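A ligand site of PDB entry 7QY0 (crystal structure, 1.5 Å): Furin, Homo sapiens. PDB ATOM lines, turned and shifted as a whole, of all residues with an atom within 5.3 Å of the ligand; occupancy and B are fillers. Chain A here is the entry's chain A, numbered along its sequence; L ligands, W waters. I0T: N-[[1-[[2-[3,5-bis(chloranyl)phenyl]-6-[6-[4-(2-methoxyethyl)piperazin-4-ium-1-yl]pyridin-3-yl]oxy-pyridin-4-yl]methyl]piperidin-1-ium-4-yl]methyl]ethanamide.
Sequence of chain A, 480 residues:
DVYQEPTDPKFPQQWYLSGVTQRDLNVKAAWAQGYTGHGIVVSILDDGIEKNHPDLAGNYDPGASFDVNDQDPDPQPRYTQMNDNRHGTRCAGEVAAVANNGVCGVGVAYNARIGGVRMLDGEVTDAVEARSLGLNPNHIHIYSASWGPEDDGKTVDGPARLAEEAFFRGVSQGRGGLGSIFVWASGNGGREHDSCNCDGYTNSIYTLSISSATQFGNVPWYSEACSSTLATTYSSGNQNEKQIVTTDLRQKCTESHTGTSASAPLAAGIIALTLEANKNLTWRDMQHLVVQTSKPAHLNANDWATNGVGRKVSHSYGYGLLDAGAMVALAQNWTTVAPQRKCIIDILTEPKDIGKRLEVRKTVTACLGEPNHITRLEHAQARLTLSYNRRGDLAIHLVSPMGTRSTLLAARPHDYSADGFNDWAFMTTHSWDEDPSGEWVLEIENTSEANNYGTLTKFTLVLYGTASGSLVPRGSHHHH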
ATOM      1  N   LEU A  45      -9.904  27.865  15.117  1.00  0.00           N
ATOM      2  CA  LEU A  45     -11.278  27.436  14.887  1.00  0.00           C
ATOM      3  C   LEU A  45     -11.961  27.322  16.250  1.00  0.00           C
ATOM      4  O   LEU A  45     -11.722  26.369  17.002  1.00  0.00           O
ATOM      5  CB  LEU A  45     -11.300  26.102  14.127  1.00  0.00           C
ATOM      6  CG  LEU A  45     -11.290  26.182  12.596  1.00  0.00           C
ATOM      7  CD1 LEU A  45     -10.146  27.042  12.137  1.00  0.00           C
ATOM      8  CD2 LEU A  45     -11.170  24.804  11.958  1.00  0.00           C
ATOM      9  N   ASP A  46     -12.803  28.297  16.592  1.00  0.00           N
ATOM     10  CA  ASP A  46     -13.347  28.363  17.948  1.00  0.00           C
ATOM     11  C   ASP A  46     -14.550  29.286  18.041  1.00  0.00           C
ATOM     12  O   ASP A  46     -15.403  29.284  17.150  1.00  0.00           O
ATOM     13  CB  ASP A  46     -12.207  28.777  18.894  1.00  0.00           C
ATOM     14  CG  ASP A  46     -12.334  28.221  20.314  1.00  0.00           C
ATOM     15  OD1 ASP A  46     -13.307  28.562  21.030  1.00  0.00           O
ATOM     16  OD2 ASP A  46     -11.436  27.461  20.742  1.00  0.00           O
ATOM     17  N   ASP A  47     -14.670  30.025  19.155  1.00  0.00           N
ATOM     18  CA  ASP A  47     -15.863  30.821  19.431  1.00  0.00           C
ATOM     19  C   ASP A  47     -15.714  32.275  18.992  1.00  0.00           C
ATOM     20  O   ASP A  47     -16.571  33.106  19.326  1.00  0.00           O
ATOM     21  CB  ASP A  47     -16.195  30.759  20.934  1.00  0.00           C
ATOM     22  CG  ASP A  47     -15.043  31.188  21.827  1.00  0.00           C
ATOM     23  OD1 ASP A  47     -14.111  31.860  21.337  1.00  0.00           O
ATOM     24  OD2 ASP A  47     -15.098  30.859  23.040  1.00  0.00           O
ATOM     25  N   ASP A  84     -18.579  33.903  27.990  1.00  0.00           N
ATOM     26  CA  ASP A  84     -18.605  32.570  27.403  1.00  0.00           C
ATOM     27  C   ASP A  84     -17.665  32.437  26.209  1.00  0.00           C
ATOM     28  O   ASP A  84     -17.091  31.370  25.987  1.00  0.00           O
ATOM     29  CB  ASP A  84     -20.009  32.229  26.921  1.00  0.00           C
ATOM     30  CG  ASP A  84     -21.017  32.226  28.001  1.00  0.00           C
ATOM     31  OD1 ASP A  84     -21.617  33.294  28.267  1.00  0.00           O
ATOM     32  OD2 ASP A  84     -21.231  31.152  28.588  1.00  0.00           O
ATOM     33  N   HIS A  87     -12.720  31.869  24.408  1.00  0.00           N
ATOM     34  CA  HIS A  87     -11.670  30.871  24.273  1.00  0.00           C
ATOM     35  C   HIS A  87     -10.824  31.106  23.029  1.00  0.00           C
ATOM     36  O   HIS A  87      -9.603  30.935  23.072  1.00  0.00           O
ATOM     37  CB  HIS A  87     -12.283  29.477  24.254  1.00  0.00           C
ATOM     38  CG  HIS A  87     -11.277  28.400  24.469  1.00  0.00           C
ATOM     39  ND1 HIS A  87     -10.696  27.696  23.435  1.00  0.00           N
ATOM     40  CD2 HIS A  87     -10.709  27.921  25.614  1.00  0.00           C
ATOM     41  CE1 HIS A  87      -9.833  26.824  23.930  1.00  0.00           C
ATOM     42  NE2 HIS A  87      -9.818  26.945  25.248  1.00  0.00           N
ATOM     43  N   MET A 119     -17.076  29.665  14.859  1.00  0.00           N
ATOM     44  CA  MET A 119     -17.872  28.511  14.465  1.00  0.00           C
ATOM     45  C   MET A 119     -18.566  27.785  15.614  1.00  0.00           C
ATOM     46  O   MET A 119     -19.502  27.022  15.356  1.00  0.00           O
ATOM     47  CB  MET A 119     -17.009  27.482  13.714  1.00  0.00           C
ATOM     48  CG  MET A 119     -15.973  26.826  14.611  1.00  0.00           C
ATOM     49  SD  MET A 119     -14.945  25.624  13.767  1.00  0.00           S
ATOM     50  CE  MET A 119     -16.176  24.364  13.522  1.00  0.00           C
ATOM     51  N   LEU A 120     -18.132  27.978  16.863  1.00  0.00           N
ATOM     52  CA  LEU A 120     -18.692  27.229  17.978  1.00  0.00           C
ATOM     53  C   LEU A 120     -19.808  27.962  18.708  1.00  0.00           C
ATOM     54  O   LEU A 120     -20.379  27.398  19.645  1.00  0.00           O
ATOM     55  CB  LEU A 120     -17.595  26.864  18.997  1.00  0.00           C
ATOM     56  CG  LEU A 120     -16.457  26.028  18.400  1.00  0.00           C
ATOM     57  CD1 LEU A 120     -15.430  25.680  19.471  1.00  0.00           C
ATOM     58  CD2 LEU A 120     -16.974  24.762  17.723  1.00  0.00           C
ATOM     59  N   VAL A 124     -23.299  23.428  15.602  1.00  0.00           N
ATOM     60  CA  VAL A 124     -22.143  22.960  14.833  1.00  0.00           C
ATOM     61  C   VAL A 124     -22.627  21.798  13.960  1.00  0.00           C
ATOM     62  O   VAL A 124     -22.791  20.671  14.439  1.00  0.00           O
ATOM     63  CB  VAL A 124     -20.982  22.564  15.731  1.00  0.00           C
ATOM     64  CG1 VAL A 124     -19.845  22.050  14.886  1.00  0.00           C
ATOM     65  CG2 VAL A 124     -20.555  23.747  16.582  1.00  0.00           C
ATOM     66  N   THR A 125     -22.854  22.083  12.694  1.00  0.00           N
ATOM     67  CA  THR A 125     -23.276  21.084  11.721  1.00  0.00           C
ATOM     68  C   THR A 125     -22.062  20.662  10.897  1.00  0.00           C
ATOM     69  O   THR A 125     -21.026  21.305  10.904  1.00  0.00           O
ATOM     70  CB  THR A 125     -24.323  21.663  10.774  1.00  0.00           C
ATOM     71  OG1 THR A 125     -23.689  22.728  10.077  1.00  0.00           O
ATOM     72  CG2 THR A 125     -25.568  22.149  11.502  1.00  0.00           C
ATOM     73  N   ASP A 126     -22.253  19.609  10.093  1.00  0.00           N
ATOM     74  CA  ASP A 126     -21.222  19.173   9.153  1.00  0.00           C
ATOM     75  C   ASP A 126     -20.838  20.287   8.188  1.00  0.00           C
ATOM     76  O   ASP A 126     -19.647  20.502   7.921  1.00  0.00           O
ATOM     77  CB  ASP A 126     -21.759  17.931   8.421  1.00  0.00           C
ATOM     78  CG  ASP A 126     -20.770  17.311   7.439  1.00  0.00           C
ATOM     79  OD1 ASP A 126     -19.551  17.230   7.740  1.00  0.00           O
ATOM     80  OD2 ASP A 126     -21.248  16.848   6.375  1.00  0.00           O
ATOM     81  N   GLU A 129     -18.651  22.824   9.954  1.00  0.00           N
ATOM     82  CA  GLU A 129     -17.304  22.304  10.113  1.00  0.00           C
ATOM     83  C   GLU A 129     -16.539  22.393   8.801  1.00  0.00           C
ATOM     84  O   GLU A 129     -15.380  22.799   8.781  1.00  0.00           O
ATOM     85  CB  GLU A 129     -17.355  20.851  10.603  1.00  0.00           C
ATOM     86  CG  GLU A 129     -17.961  20.711  11.981  1.00  0.00           C
ATOM     87  CD  GLU A 129     -18.015  19.260  12.449  1.00  0.00           C
ATOM     88  OE1 GLU A 129     -17.364  18.395  11.831  1.00  0.00           O
ATOM     89  OE2 GLU A 129     -18.738  18.998  13.439  1.00  0.00           O
ATOM     90  N   LEU A 133     -12.972  24.343   8.220  1.00  0.00           N
ATOM     91  CA  LEU A 133     -11.738  23.661   7.841  1.00  0.00           C
ATOM     92  C   LEU A 133     -11.257  24.094   6.480  1.00  0.00           C
ATOM     93  O   LEU A 133     -10.049  24.117   6.228  1.00  0.00           O
ATOM     94  CB  LEU A 133     -11.959  22.143   7.835  1.00  0.00           C
ATOM     95  CG  LEU A 133     -12.223  21.529   9.209  1.00  0.00           C
ATOM     96  CD1 LEU A 133     -12.835  20.118   9.055  1.00  0.00           C
ATOM     97  CD2 LEU A 133     -10.982  21.467  10.081  1.00  0.00           C
ATOM     98  N   ALA A 145      -7.457  23.666  16.228  1.00  0.00           N
ATOM     99  CA  ALA A 145      -8.783  23.313  16.739  1.00  0.00           C
ATOM    100  C   ALA A 145      -8.641  22.583  18.067  1.00  0.00           C
ATOM    101  O   ALA A 145      -7.944  21.568  18.160  1.00  0.00           O
ATOM    102  CB  ALA A 145      -9.548  22.444  15.734  1.00  0.00           C
ATOM    103  N   SER A 146      -9.329  23.087  19.088  1.00  0.00           N
ATOM    104  CA  SER A 146      -9.136  22.592  20.440  1.00  0.00           C
ATOM    105  C   SER A 146     -10.273  21.702  20.927  1.00  0.00           C
ATOM    106  O   SER A 146     -10.242  21.263  22.083  1.00  0.00           O
ATOM    107  CB  SER A 146      -8.953  23.767  21.402  1.00  0.00           C
ATOM    108  OG  SER A 146      -7.665  24.333  21.227  1.00  0.00           O
ATOM    109  N   TRP A 147     -11.214  21.364  20.062  1.00  0.00           N
ATOM    110  CA  TRP A 147     -12.452  20.714  20.487  1.00  0.00           C
ATOM    111  C   TRP A 147     -12.925  19.725  19.421  1.00  0.00           C
ATOM    112  O   TRP A 147     -12.461  19.712  18.291  1.00  0.00           O
ATOM    113  CB  TRP A 147     -13.549  21.754  20.746  1.00  0.00           C
ATOM    114  CG  TRP A 147     -13.150  22.953  21.552  1.00  0.00           C
ATOM    115  CD1 TRP A 147     -12.801  24.181  21.064  1.00  0.00           C
ATOM    116  CD2 TRP A 147     -13.069  23.049  22.985  1.00  0.00           C
ATOM    117  NE1 TRP A 147     -12.511  25.041  22.108  1.00  0.00           N
ATOM    118  CE2 TRP A 147     -12.659  24.366  23.292  1.00  0.00           C
ATOM    119  CE3 TRP A 147     -13.302  22.159  24.043  1.00  0.00           C
ATOM    120  CZ2 TRP A 147     -12.482  24.819  24.601  1.00  0.00           C
ATOM    121  CZ3 TRP A 147     -13.104  22.607  25.344  1.00  0.00           C
ATOM    122  CH2 TRP A 147     -12.698  23.924  25.615  1.00  0.00           C
ATOM    123  N   GLY A 148     -13.902  18.917  19.817  1.00  0.00           N
ATOM    124  CA  GLY A 148     -14.503  17.943  18.937  1.00  0.00           C
ATOM    125  C   GLY A 148     -15.814  17.436  19.512  1.00  0.00           C
ATOM    126  O   GLY A 148     -16.537  18.174  20.195  1.00  0.00           O
ATOM    127  N   PRO A 149     -16.124  16.164  19.263  1.00  0.00           N
ATOM    128  CA  PRO A 149     -17.311  15.558  19.878  1.00  0.00           C
ATOM    129  C   PRO A 149     -17.196  15.574  21.397  1.00  0.00           C
ATOM    130  O   PRO A 149     -16.125  15.717  21.966  1.00  0.00           O
ATOM    131  CB  PRO A 149     -17.322  14.122  19.353  1.00  0.00           C
ATOM    132  CG  PRO A 149     -16.233  14.025  18.395  1.00  0.00           C
ATOM    133  CD  PRO A 149     -15.319  15.178  18.528  1.00  0.00           C
ATOM    134  N   ASP A 157     -17.708   9.547  17.626  1.00  0.00           N
ATOM    135  CA  ASP A 157     -18.129  10.332  16.471  1.00  0.00           C
ATOM    136  C   ASP A 157     -16.904  11.015  15.874  1.00  0.00           C
ATOM    137  O   ASP A 157     -15.863  11.142  16.514  1.00  0.00           O
ATOM    138  CB  ASP A 157     -19.182  11.366  16.851  1.00  0.00           C
ATOM    139  CG  ASP A 157     -20.110  11.740  15.690  1.00  0.00           C
ATOM    140  OD1 ASP A 157     -19.994  11.181  14.564  1.00  0.00           O
ATOM    141  OD2 ASP A 157     -20.982  12.602  15.926  1.00  0.00           O
ATOM    142  N   GLY A 158     -17.088  11.476  14.644  1.00  0.00           N
ATOM    143  CA  GLY A 158     -16.032  12.103  13.888  1.00  0.00           C
ATOM    144  C   GLY A 158     -16.621  12.936  12.778  1.00  0.00           C
ATOM    145  O   GLY A 158     -17.843  13.152  12.704  1.00  0.00           O
ATOM    146  N   PRO A 159     -15.758  13.436  11.893  1.00  0.00           N
ATOM    147  CA  PRO A 159     -16.243  14.259  10.777  1.00  0.00           C
ATOM    148  C   PRO A 159     -17.215  13.476   9.913  1.00  0.00           C
ATOM    149  O   PRO A 159     -16.947  12.329   9.546  1.00  0.00           O
ATOM    150  CB  PRO A 159     -14.964  14.615  10.009  1.00  0.00           C
ATOM    151  CG  PRO A 159     -13.945  13.586  10.438  1.00  0.00           C
ATOM    152  CD  PRO A 159     -14.298  13.265  11.870  1.00  0.00           C
ATOM    153  N   ALA A 160     -18.348  14.097   9.627  1.00  0.00           N
ATOM    154  CA  ALA A 160     -19.303  13.604   8.648  1.00  0.00           C
ATOM    155  C   ALA A 160     -18.765  13.941   7.259  1.00  0.00           C
ATOM    156  O   ALA A 160     -17.609  14.345   7.103  1.00  0.00           O
ATOM    157  CB  ALA A 160     -20.686  14.169   8.944  1.00  0.00           C
ATOM    158  N   TRP A 184      -4.677  19.573  16.246  1.00  0.00           N
ATOM    159  CA  TRP A 184      -5.838  19.204  17.053  1.00  0.00           C
ATOM    160  C   TRP A 184      -5.457  18.901  18.493  1.00  0.00           C
ATOM    161  O   TRP A 184      -4.396  18.327  18.753  1.00  0.00           O
ATOM    162  CB  TRP A 184      -6.594  17.960  16.479  1.00  0.00           C
ATOM    163  CG  TRP A 184      -8.070  18.199  16.453  1.00  0.00           C
ATOM    164  CD1 TRP A 184      -8.979  17.942  17.439  1.00  0.00           C
ATOM    165  CD2 TRP A 184      -8.796  18.799  15.388  1.00  0.00           C
ATOM    166  NE1 TRP A 184     -10.225  18.347  17.057  1.00  0.00           N
ATOM    167  CE2 TRP A 184     -10.150  18.876  15.790  1.00  0.00           C
ATOM    168  CE3 TRP A 184      -8.446  19.274  14.122  1.00  0.00           C
ATOM    169  CZ2 TRP A 184     -11.143  19.394  14.974  1.00  0.00           C
ATOM    170  CZ3 TRP A 184      -9.427  19.796  13.319  1.00  0.00           C
ATOM    171  CH2 TRP A 184     -10.756  19.852  13.737  1.00  0.00           C
ATOM    172  N   TYR A 201     -11.815  13.311  14.895  1.00  0.00           N
ATOM    173  CA  TYR A 201     -11.003  14.448  14.475  1.00  0.00           C
ATOM    174  C   TYR A 201      -9.555  14.245  14.900  1.00  0.00           C
ATOM    175  O   TYR A 201      -8.649  14.266  14.075  1.00  0.00           O
ATOM    176  CB  TYR A 201     -11.577  15.751  15.041  1.00  0.00           C
ATOM    177  CG  TYR A 201     -12.994  15.991  14.586  1.00  0.00           C
ATOM    178  CD1 TYR A 201     -14.048  15.341  15.216  1.00  0.00           C
ATOM    179  CD2 TYR A 201     -13.292  16.814  13.502  1.00  0.00           C
ATOM    180  CE1 TYR A 201     -15.335  15.506  14.803  1.00  0.00           C
ATOM    181  CE2 TYR A 201     -14.603  16.994  13.081  1.00  0.00           C
ATOM    182  CZ  TYR A 201     -15.622  16.335  13.746  1.00  0.00           C
ATOM    183  OH  TYR A 201     -16.921  16.471  13.354  1.00  0.00           O
HETATM  184  CAA I0T L   1     -24.140  13.091  10.346  1.00  0.00           C
HETATM  185  CAB I0T L   1     -23.799  14.553  10.644  1.00  0.00           C
HETATM  186  CAE I0T L   1     -22.847  16.145  12.206  1.00  0.00           C
HETATM  187  CAF I0T L   1     -21.981  16.096  13.452  1.00  0.00           C
HETATM  188  CAG I0T L   1     -20.619  15.475  13.147  1.00  0.00           C
HETATM  189  CAH I0T L   1     -19.746  15.511  14.413  1.00  0.00           C
HETATM  190  CAJ I0T L   1     -20.841  17.540  15.204  1.00  0.00           C
HETATM  191  CAK I0T L   1     -21.748  17.539  13.970  1.00  0.00           C
HETATM  192  CAL I0T L   1     -18.712  16.769  16.185  1.00  0.00           C
HETATM  193  CAM I0T L   1     -18.261  18.139  16.703  1.00  0.00           C
HETATM  194  CAN I0T L   1     -18.949  18.764  17.744  1.00  0.00           C
HETATM  195  CAO I0T L   1     -18.491  19.997  18.180  1.00  0.00           C
HETATM  196  CAQ I0T L   1     -16.751  20.041  16.621  1.00  0.00           C
HETATM  197  CAR I0T L   1     -17.158  18.790  16.149  1.00  0.00           C
HETATM  198  CAS I0T L   1     -15.668  20.747  16.072  1.00  0.00           C
HETATM  199  CAT I0T L   1     -14.939  21.672  16.816  1.00  0.00           C
HETATM  200  CAU I0T L   1     -13.902  22.386  16.233  1.00  0.00           C
HETATM  201  CAW I0T L   1     -13.591  22.209  14.891  1.00  0.00           C
HETATM  202  CAX I0T L   1     -14.342  21.334  14.124  1.00  0.00           C
HETATM  203  CAZ I0T L   1     -15.377  20.607  14.710  1.00  0.00           C
HETATM  204  CBB I0T L   1     -18.646  21.559  19.968  1.00  0.00           C
HETATM  205  CBC I0T L   1     -19.482  22.630  20.227  1.00  0.00           C
HETATM  206  CBD I0T L   1     -19.074  23.632  21.070  1.00  0.00           C
HETATM  207  CBE I0T L   1     -17.820  23.576  21.673  1.00  0.00           C
HETATM  208  CBG I0T L   1     -17.406  21.480  20.584  1.00  0.00           C
HETATM  209  CBI I0T L   1     -18.334  25.678  22.789  1.00  0.00           C
HETATM  210  CBJ I0T L   1     -18.192  26.206  24.194  1.00  0.00           C
HETATM  211  CBL I0T L   1     -16.788  26.857  26.002  1.00  0.00           C
HETATM  212  CBM I0T L   1     -15.429  27.520  26.209  1.00  0.00           C
HETATM  213  CBO I0T L   1     -13.810  27.512  27.818  1.00  0.00           C
HETATM  214  CBP I0T L   1     -16.295  24.925  24.674  1.00  0.00           C
HETATM  215  CBQ I0T L   1     -16.183  24.404  23.267  1.00  0.00           C
HETATM  216  NAD I0T L   1     -23.207  14.786  11.810  1.00  0.00           N
HETATM  217  NAI I0T L   1     -19.538  16.879  14.946  1.00  0.00           N
HETATM  218  NAP I0T L   1     -17.442  20.607  17.623  1.00  0.00           N
HETATM  219  NBF I0T L   1     -17.015  22.524  21.435  1.00  0.00           N
HETATM  220  NBH I0T L   1     -17.445  24.543  22.525  1.00  0.00           N
HETATM  221  NBK I0T L   1     -16.804  26.291  24.654  1.00  0.00           N
HETATM  222  OAC I0T L   1     -24.080  15.429   9.837  1.00  0.00           O
HETATM  223  OBA I0T L   1     -19.171  20.608  19.173  1.00  0.00           O
HETATM  224  OBN I0T L   1     -14.610  26.655  27.001  1.00  0.00           O
HETATM  225 CL1  I0T L   1     -12.975  23.500  17.159  1.00  0.00          CL
HETATM  226 CL2  I0T L   1     -14.001  21.137  12.431  1.00  0.00          CL
HETATM  227  O   HOH W   1     -22.944  12.714  13.935  1.00  0.00           O
HETATM  228  O   HOH W   2     -17.187  29.411  24.024  1.00  0.00           O
HETATM  229  O   HOH W   3     -15.103  27.926  22.988  1.00  0.00           O
HETATM  230  O   HOH W   4     -12.176  29.738  28.467  1.00  0.00           O
HETATM  231  O   HOH W   5     -18.496  18.601  21.974  1.00  0.00           O
HETATM  232  O   HOH W   6     -20.954  14.645  17.777  1.00  0.00           O
HETATM  233  O   HOH W   7     -24.779  18.077  10.197  1.00  0.00           O
HETATM  234  O   HOH W   8     -11.549  25.960  28.991  1.00  0.00           O
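NAI of the ligand lies within salt-bridge range of OE2 of Glu 129 (2.7 Å). OH of Tyr 201 is in hydrogen-bond range of NAI of the ligand, 3.1 Å away.
Water W7 bridges an oxygen (OAC) of the ligand and the backbone NH (N) of Asp 126. Water W3 lies within hydrogen-bond range of the side-chain carboxylate of Asp 46 (2.7 Å), a nitrogen (NBK) of the ligand (2.9 Å) and the side-chain carboxylate of Asp 47 (2.9 Å). Water W1 lies within hydrogen-bond range of the side-chain carboxylate (OD2) of Asp 157 (2.8 Å) and a nitrogen (NAD) of the ligand (3.0 Å). Water W2 lies within hydrogen-bond range of the side-chain carboxylate (OD2) of Asp 47 (2.7 Å), the backbone carbonyl oxygen (O) of Asp 84 (2.8 Å) and a nitrogen (NBK) of the ligand (3.2 Å).
N of Leu 120 is in hydrogen-bond range of O of Asp 46 (3.0 Å). OD2 of Asp 46 sits at hydrogen-bond distance from ND1 of His 87 (2.8 Å). The indole nitrogen of Trp 147 lies within hydrogen-bond range of the side-chain carboxylate of Asp 46, at 3.0 Å. The backbone NH (N) of Met 119 is in hydrogen-bond range of the backbone carbonyl oxygen (O) of Asp 46, 2.9 Å away. OE1 of Glu 129 lies within hydrogen-bond range of OH of Tyr 201, 2.5 Å away. NE1 of Trp 147 is in hydrogen-bond range of ND1 of His 87 (3.5 Å). The side-chain carboxylate (OD2) of Asp 47 sits at hydrogen-bond distance from the backbone NH (N) of His 87 (2.9 Å). NE1 of Trp 184 is in hydrogen-bond range of O of Trp 147, 2.9 Å away.
Leu 45 touches the ligand. His 87 touches the ligand (CD2 to CBO, 3.8 Å). CE of Met 119 touches CAX of the ligand (3.6 Å). Leu 120 touches the ligand. Val 124 touches the ligand (O to CAK, 3.3 Å). Asp 126 touches the ligand (CB to OAC, 3.7 Å). CG of Leu 133 touches CL2 of the ligand, at 3.7 Å. Ala 145 touches the ligand (CB to CL1, 3.9 Å). Trp 147 touches the ligand. Gly 148 touches the ligand (O to CAO, 3.3 Å). Pro 149 touches the ligand (N to CAM, 3.9 Å). Asp 157 touches the ligand. O of Gly 158 touches CAH of the ligand (3.5 Å). Ala 160 touches the ligand (CB to CAB, 3.6 Å). Trp 184 touches the ligand. Hydrophobic or aromatic side chains that line the ligand: His 87, Met 119, Leu 120, Val 124, Leu 133, Ala 145, Trp 147, Ala 160, Trp 184 and Tyr 201. The nearest printed residue that does not touch the ligand is Ser 146 (4.1 Å).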
